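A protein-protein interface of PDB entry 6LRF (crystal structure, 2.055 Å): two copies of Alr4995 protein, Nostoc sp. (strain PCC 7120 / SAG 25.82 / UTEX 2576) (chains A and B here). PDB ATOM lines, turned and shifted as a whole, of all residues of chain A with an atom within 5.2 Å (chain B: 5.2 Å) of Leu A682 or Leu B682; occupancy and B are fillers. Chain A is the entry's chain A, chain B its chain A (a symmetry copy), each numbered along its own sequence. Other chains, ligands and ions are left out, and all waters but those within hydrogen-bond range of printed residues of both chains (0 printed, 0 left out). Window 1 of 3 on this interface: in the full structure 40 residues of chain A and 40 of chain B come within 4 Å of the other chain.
Glu A467 touches Asp B679, and with the chains exchanged Asp A679 touches Glu B467.
Glu A467 touches Leu B682, and with the chains exchanged Leu A682 touches Glu B467.
Glu A467 touches Ser B685, and with the chains exchanged Ser A685 touches Glu B467.
Leu A682 touches its own counterpart, Leu B682.
Of the 9 pairs that touch across the chains among the printed residues, 9 have their exchanged pair printed and touching as well.
N of Gly B681 lies within hydrogen-bond range of OD2 of Asp B679, 2.8 Å away.
The side-chain carboxylate of Asp B679 is in hydrogen-bond range of the backbone NH of Leu B682 (3.1 Å).
The side-chain carboxylate (OD2) of Asp A679 lies within hydrogen-bond range of the backbone NH (N) of Leu A682, 3.1 Å away.
The side-chain carboxylate of Asp A679 lies within hydrogen-bond range of the backbone NH of Gly A681 (2.8 Å).
Among the printed residues, merely in contact across the chains: Leu A682 with Leu B682 (3.9 Å), Glu A467 with Ser B685 (3.9 Å), Ser A685 with Glu B467 (3.9 Å), Leu A682 with Glu B467 (3.997 Å) and Glu A467 with Leu B682 (3.998 Å).
The side-chain carboxylate (OD1) of Asp A679 is in hydrogen-bond range of the backbone NH (N) of Glu B467 (3.4 Å).
The side-chain carboxylate of Glu B467 lies close to the backbone carbonyl oxygen of Gly A681 (3.3 Å).
N of Glu A467 lies within hydrogen-bond range of OD1 of Asp B679, 3.4 Å away.
The side-chain carboxylate of Glu A467 lies close to the backbone carbonyl oxygen of Gly B681 (3.3 Å).
Of the printed residues of chain B, Leu A682 touches Glu B467 and Leu B682.
Printed residues of chain A within 4 Å of Leu B682: Glu A467 and Leu A682.
Printed residues of chain A within 4 Å of Ser B685: Glu A467.
Printed residues of chain A within 4 Å of Glu B467: Asp A679, Gly A681, Leu A682 and Ser A685.
Printed residues of chain B within 4 Å of Asp A679: Glu B467.
The nearest printed residue of chain A that does not touch Leu B682 is Leu A686 (4.7 Å).
The nearest printed residue of chain B that does not touch Glu A467 is Val B680 (5.6 Å).
Printed residues of chain B that touch a printed residue of chain A: Glu B467, Asp B679, Gly B681, Leu B682 and Ser B685.
Among the printed residues, 9 pairs touch across the chains.
Among the printed residues, no Asp or Glu carboxylate lies within 4 Å of a Lys or Arg side-chain nitrogen of the other chain.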
ATOM      1  N   GLU A 467      24.892  22.001 -29.082  1.00  0.00           N
ATOM      2  CA  GLU A 467      23.507  21.599 -29.318  1.00  0.00           C
ATOM      3  C   GLU A 467      23.491  20.367 -30.205  1.00  0.00           C
ATOM      4  O   GLU A 467      22.771  19.417 -29.922  1.00  0.00           O
ATOM      5  CB  GLU A 467      22.676  22.714 -29.961  1.00  0.00           C
ATOM      6  CG  GLU A 467      21.194  22.334 -30.180  1.00  0.00           C
ATOM      7  CD  GLU A 467      20.438  23.311 -31.094  1.00  0.00           C
ATOM      8  OE1 GLU A 467      19.314  22.966 -31.531  1.00  0.00           O
ATOM      9  OE2 GLU A 467      20.968  24.421 -31.384  1.00  0.00           O
ATOM     10  N   VAL A 470      24.494  16.917 -28.190  1.00  0.00           N
ATOM     11  CA  VAL A 470      23.480  16.432 -27.271  1.00  0.00           C
ATOM     12  C   VAL A 470      22.353  15.795 -28.055  1.00  0.00           C
ATOM     13  O   VAL A 470      21.949  14.677 -27.774  1.00  0.00           O
ATOM     14  CB  VAL A 470      22.934  17.581 -26.395  1.00  0.00           C
ATOM     15  CG1 VAL A 470      21.752  17.109 -25.562  1.00  0.00           C
ATOM     16  CG2 VAL A 470      24.039  18.121 -25.510  1.00  0.00           C
ATOM     17  N   THR A 678      26.406  17.513 -19.858  1.00  0.00           N
ATOM     18  CA  THR A 678      25.177  18.302 -19.924  1.00  0.00           C
ATOM     19  C   THR A 678      24.357  18.058 -18.657  1.00  0.00           C
ATOM     20  O   THR A 678      24.667  17.155 -17.879  1.00  0.00           O
ATOM     21  CB  THR A 678      24.355  17.960 -21.209  1.00  0.00           C
ATOM     22  OG1 THR A 678      23.442  19.020 -21.528  1.00  0.00           O
ATOM     23  CG2 THR A 678      23.590  16.650 -21.069  1.00  0.00           C
ATOM     24  N   ASP A 679      23.346  18.892 -18.427  1.00  0.00           N
ATOM     25  CA  ASP A 679      22.417  18.705 -17.307  1.00  0.00           C
ATOM     26  C   ASP A 679      21.633  17.402 -17.506  1.00  0.00           C
ATOM     27  O   ASP A 679      21.049  17.185 -18.572  1.00  0.00           O
ATOM     28  CB  ASP A 679      21.467  19.908 -17.205  1.00  0.00           C
ATOM     29  CG  ASP A 679      20.529  19.836 -15.994  1.00  0.00           C
ATOM     30  OD1 ASP A 679      20.772  20.566 -15.009  1.00  0.00           O
ATOM     31  OD2 ASP A 679      19.530  19.084 -16.033  1.00  0.00           O
ATOM     32  N   VAL A 680      21.608  16.531 -16.501  1.00  0.00           N
ATOM     33  CA  VAL A 680      20.978  15.225 -16.702  1.00  0.00           C
ATOM     34  C   VAL A 680      19.461  15.337 -16.820  1.00  0.00           C
ATOM     35  O   VAL A 680      18.818  14.486 -17.436  1.00  0.00           O
ATOM     36  CB  VAL A 680      21.332  14.244 -15.574  1.00  0.00           C
ATOM     37  CG1 VAL A 680      20.654  14.660 -14.262  1.00  0.00           C
ATOM     38  CG2 VAL A 680      20.946  12.823 -15.961  1.00  0.00           C
ATOM     39  N   GLY A 681      18.883  16.393 -16.250  1.00  0.00           N
ATOM     40  CA  GLY A 681      17.445  16.576 -16.338  1.00  0.00           C
ATOM     41  C   GLY A 681      17.071  16.968 -17.760  1.00  0.00           C
ATOM     42  O   GLY A 681      16.111  16.460 -18.333  1.00  0.00           O
ATOM     43  N   LEU A 682      17.844  17.886 -18.319  1.00  0.00           N
ATOM     44  CA  LEU A 682      17.686  18.292 -19.717  1.00  0.00           C
ATOM     45  C   LEU A 682      17.833  17.087 -20.661  1.00  0.00           C
ATOM     46  O   LEU A 682      17.032  16.902 -21.579  1.00  0.00           O
ATOM     47  CB  LEU A 682      18.714  19.382 -20.047  1.00  0.00           C
ATOM     48  CG  LEU A 682      18.757  20.092 -21.402  1.00  0.00           C
ATOM     49  CD1 LEU A 682      19.762  19.412 -22.319  1.00  0.00           C
ATOM     50  CD2 LEU A 682      17.371  20.201 -22.050  1.00  0.00           C
ATOM     51  N   PHE A 683      18.854  16.269 -20.413  1.00  0.00           N
ATOM     52  CA  PHE A 683      19.106  15.083 -21.219  1.00  0.00           C
ATOM     53  C   PHE A 683      17.928  14.130 -21.153  1.00  0.00           C
ATOM     54  O   PHE A 683      17.451  13.634 -22.180  1.00  0.00           O
ATOM     55  CB  PHE A 683      20.383  14.369 -20.755  1.00  0.00           C
ATOM     56  CG  PHE A 683      20.618  13.050 -21.441  1.00  0.00           C
ATOM     57  CD1 PHE A 683      21.335  12.991 -22.623  1.00  0.00           C
ATOM     58  CD2 PHE A 683      20.111  11.872 -20.910  1.00  0.00           C
ATOM     59  CE1 PHE A 683      21.538  11.777 -23.262  1.00  0.00           C
ATOM     60  CE2 PHE A 683      20.307  10.663 -21.550  1.00  0.00           C
ATOM     61  CZ  PHE A 683      21.026  10.622 -22.728  1.00  0.00           C
ATOM     62  N   LEU A 684      17.453  13.872 -19.937  1.00  0.00           N
ATOM     63  CA  LEU A 684      16.314  12.991 -19.744  1.00  0.00           C
ATOM     64  C   LEU A 684      15.049  13.556 -20.410  1.00  0.00           C
ATOM     65  O   LEU A 684      14.234  12.819 -20.956  1.00  0.00           O
ATOM     66  CB  LEU A 684      16.084  12.757 -18.245  1.00  0.00           C
ATOM     67  CG  LEU A 684      17.081  11.796 -17.600  1.00  0.00           C
ATOM     68  CD1 LEU A 684      16.809  11.665 -16.105  1.00  0.00           C
ATOM     69  CD2 LEU A 684      17.014  10.432 -18.288  1.00  0.00           C
ATOM     70  N   SER A 685      14.907  14.875 -20.360  1.00  0.00           N
ATOM     71  CA  SER A 685      13.793  15.570 -20.984  1.00  0.00           C
ATOM     72  C   SER A 685      13.803  15.392 -22.512  1.00  0.00           C
ATOM     73  O   SER A 685      12.778  15.081 -23.120  1.00  0.00           O
ATOM     74  CB  SER A 685      13.844  17.059 -20.627  1.00  0.00           C
ATOM     75  OG  SER A 685      12.778  17.759 -21.235  1.00  0.00           O
ATOM     76  N   LEU A 686      14.965  15.598 -23.123  1.00  0.00           N
ATOM     77  CA  LEU A 686      15.108  15.392 -24.556  1.00  0.00           C
ATOM     78  C   LEU A 686      14.923  13.913 -24.914  1.00  0.00           C
ATOM     79  O   LEU A 686      14.374  13.586 -25.973  1.00  0.00           O
ATOM     80  CB  LEU A 686      16.474  15.882 -25.029  1.00  0.00           C
ATOM     81  CG  LEU A 686      16.730  17.378 -24.936  1.00  0.00           C
ATOM     82  CD1 LEU A 686      18.126  17.686 -25.417  1.00  0.00           C
ATOM     83  CD2 LEU A 686      15.718  18.094 -25.785  1.00  0.00           C
ATOM     84  N   LEU A 687      15.370  13.020 -24.033  1.00  0.00           N
ATOM     85  CA  LEU A 687      15.287  11.582 -24.310  1.00  0.00           C
ATOM     86  C   LEU A 687      13.847  11.095 -24.355  1.00  0.00           C
ATOM     87  O   LEU A 687      13.476  10.353 -25.268  1.00  0.00           O
ATOM     88  CB  LEU A 687      16.058  10.771 -23.260  1.00  0.00           C
ATOM     89  CG  LEU A 687      16.050   9.241 -23.397  1.00  0.00           C
ATOM     90  CD1 LEU A 687      16.800   8.810 -24.671  1.00  0.00           C
ATOM     91  CD2 LEU A 687      16.660   8.560 -22.152  1.00  0.00           C
ATOM     92  N   GLU B 467      17.799  22.130 -14.686  1.00  0.00           N
ATOM     93  CA  GLU B 467      16.720  21.975 -15.658  1.00  0.00           C
ATOM     94  C   GLU B 467      15.607  22.953 -15.326  1.00  0.00           C
ATOM     95  O   GLU B 467      15.095  23.625 -16.213  1.00  0.00           O
ATOM     96  CB  GLU B 467      16.165  20.549 -15.697  1.00  0.00           C
ATOM     97  CG  GLU B 467      15.053  20.344 -16.751  1.00  0.00           C
ATOM     98  CD  GLU B 467      14.285  19.022 -16.583  1.00  0.00           C
ATOM     99  OE1 GLU B 467      13.216  18.874 -17.222  1.00  0.00           O
ATOM    100  OE2 GLU B 467      14.744  18.136 -15.809  1.00  0.00           O
ATOM    101  N   VAL B 470      16.484  26.827 -16.419  1.00  0.00           N
ATOM    102  CA  VAL B 470      16.457  27.077 -17.848  1.00  0.00           C
ATOM    103  C   VAL B 470      15.021  27.137 -18.323  1.00  0.00           C
ATOM    104  O   VAL B 470      14.622  28.074 -18.997  1.00  0.00           O
ATOM    105  CB  VAL B 470      17.223  25.978 -18.616  1.00  0.00           C
ATOM    106  CG1 VAL B 470      17.044  26.144 -20.118  1.00  0.00           C
ATOM    107  CG2 VAL B 470      18.691  26.018 -18.239  1.00  0.00           C
ATOM    108  N   THR B 678      24.071  28.373 -20.089  1.00  0.00           N
ATOM    109  CA  THR B 678      23.623  27.206 -20.847  1.00  0.00           C
ATOM    110  C   THR B 678      24.050  27.362 -22.306  1.00  0.00           C
ATOM    111  O   THR B 678      24.496  28.435 -22.714  1.00  0.00           O
ATOM    112  CB  THR B 678      22.075  27.014 -20.724  1.00  0.00           C
ATOM    113  OG1 THR B 678      21.703  25.664 -21.037  1.00  0.00           O
ATOM    114  CG2 THR B 678      21.305  27.977 -21.618  1.00  0.00           C
ATOM    115  N   ASP B 679      23.962  26.280 -23.076  1.00  0.00           N
ATOM    116  CA  ASP B 679      24.238  26.320 -24.517  1.00  0.00           C
ATOM    117  C   ASP B 679      23.202  27.212 -25.210  1.00  0.00           C
ATOM    118  O   ASP B 679      21.996  27.026 -25.023  1.00  0.00           O
ATOM    119  CB  ASP B 679      24.214  24.897 -25.096  1.00  0.00           C
ATOM    120  CG  ASP B 679      24.594  24.843 -26.580  1.00  0.00           C
ATOM    121  OD1 ASP B 679      25.731  24.424 -26.889  1.00  0.00           O
ATOM    122  OD2 ASP B 679      23.754  25.181 -27.444  1.00  0.00           O
ATOM    123  N   VAL B 680      23.647  28.178 -26.009  1.00  0.00           N
ATOM    124  CA  VAL B 680      22.693  29.127 -26.585  1.00  0.00           C
ATOM    125  C   VAL B 680      21.811  28.474 -27.645  1.00  0.00           C
ATOM    126  O   VAL B 680      20.692  28.927 -27.893  1.00  0.00           O
ATOM    127  CB  VAL B 680      23.402  30.347 -27.192  1.00  0.00           C
ATOM    128  CG1 VAL B 680      24.172  29.953 -28.459  1.00  0.00           C
ATOM    129  CG2 VAL B 680      22.400  31.456 -27.486  1.00  0.00           C
ATOM    130  N   GLY B 681      22.295  27.397 -28.261  1.00  0.00           N
ATOM    131  CA  GLY B 681      21.503  26.710 -29.266  1.00  0.00           C
ATOM    132  C   GLY B 681      20.355  25.976 -28.592  1.00  0.00           C
ATOM    133  O   GLY B 681      19.215  26.009 -29.048  1.00  0.00           O
ATOM    134  N   LEU B 682      20.675  25.304 -27.496  1.00  0.00           N
ATOM    135  CA  LEU B 682      19.668  24.635 -26.670  1.00  0.00           C
ATOM    136  C   LEU B 682      18.610  25.634 -26.173  1.00  0.00           C
ATOM    137  O   LEU B 682      17.409  25.369 -26.238  1.00  0.00           O
ATOM    138  CB  LEU B 682      20.362  23.933 -25.496  1.00  0.00           C
ATOM    139  CG  LEU B 682      19.603  23.062 -24.491  1.00  0.00           C
ATOM    140  CD1 LEU B 682      19.220  23.882 -23.270  1.00  0.00           C
ATOM    141  CD2 LEU B 682      18.389  22.367 -25.119  1.00  0.00           C
ATOM    142  N   PHE B 683      19.073  26.787 -25.692  1.00  0.00           N
ATOM    143  CA  PHE B 683      18.185  27.830 -25.199  1.00  0.00           C
ATOM    144  C   PHE B 683      17.256  28.309 -26.298  1.00  0.00           C
ATOM    145  O   PHE B 683      16.040  28.422 -26.102  1.00  0.00           O
ATOM    146  CB  PHE B 683      18.988  29.012 -24.642  1.00  0.00           C
ATOM    147  CG  PHE B 683      18.135  30.192 -24.259  1.00  0.00           C
ATOM    148  CD1 PHE B 683      17.610  30.295 -22.984  1.00  0.00           C
ATOM    149  CD2 PHE B 683      17.849  31.192 -25.179  1.00  0.00           C
ATOM    150  CE1 PHE B 683      16.812  31.375 -22.636  1.00  0.00           C
ATOM    151  CE2 PHE B 683      17.049  32.264 -24.836  1.00  0.00           C
ATOM    152  CZ  PHE B 683      16.534  32.352 -23.558  1.00  0.00           C
ATOM    153  N   LEU B 684      17.829  28.588 -27.466  1.00  0.00           N
ATOM    154  CA  LEU B 684      17.044  29.035 -28.604  1.00  0.00           C
ATOM    155  C   LEU B 684      16.041  27.959 -29.051  1.00  0.00           C
ATOM    156  O   LEU B 684      14.922  28.260 -29.454  1.00  0.00           O
ATOM    157  CB  LEU B 684      17.974  29.427 -29.759  1.00  0.00           C
ATOM    158  CG  LEU B 684      18.677  30.772 -29.571  1.00  0.00           C
ATOM    159  CD1 LEU B 684      19.617  31.053 -30.737  1.00  0.00           C
ATOM    160  CD2 LEU B 684      17.640  31.886 -29.423  1.00  0.00           C
ATOM    161  N   SER B 685      16.462  26.702 -28.963  1.00  0.00           N
ATOM    162  CA  SER B 685      15.619  25.567 -29.300  1.00  0.00           C
ATOM    163  C   SER B 685      14.402  25.472 -28.365  1.00  0.00           C
ATOM    164  O   SER B 685      13.269  25.296 -28.815  1.00  0.00           O
ATOM    165  CB  SER B 685      16.439  24.274 -29.230  1.00  0.00           C
ATOM    166  OG  SER B 685      15.636  23.153 -29.539  1.00  0.00           O
ATOM    167  N   LEU B 686      14.646  25.583 -27.063  1.00  0.00           N
ATOM    168  CA  LEU B 686      13.565  25.577 -26.090  1.00  0.00           C
ATOM    169  C   LEU B 686      12.675  26.814 -26.260  1.00  0.00           C
ATOM    170  O   LEU B 686      11.455  26.742 -26.069  1.00  0.00           O
ATOM    171  CB  LEU B 686      14.126  25.523 -24.672  1.00  0.00           C
ATOM    172  CG  LEU B 686      14.859  24.250 -24.280  1.00  0.00           C
ATOM    173  CD1 LEU B 686      15.367  24.371 -22.865  1.00  0.00           C
ATOM    174  CD2 LEU B 686      13.909  23.090 -24.394  1.00  0.00           C
ATOM    175  N   LEU B 687      13.277  27.944 -26.626  1.00  0.00           N
ATOM    176  CA  LEU B 687      12.520  29.193 -26.762  1.00  0.00           C
ATOM    177  C   LEU B 687      11.525  29.131 -27.911  1.00  0.00           C
ATOM    178  O   LEU B 687      10.369  29.528 -27.747  1.00  0.00           O
ATOM    179  CB  LEU B 687      13.456  30.388 -26.973  1.00  0.00           C
ATOM    180  CG  LEU B 687      12.814  31.771 -27.155  1.00  0.00           C
ATOM    181  CD1 LEU B 687      12.107  32.213 -25.861  1.00  0.00           C
ATOM    182  CD2 LEU B 687      13.857  32.825 -27.589  1.00  0.00           C
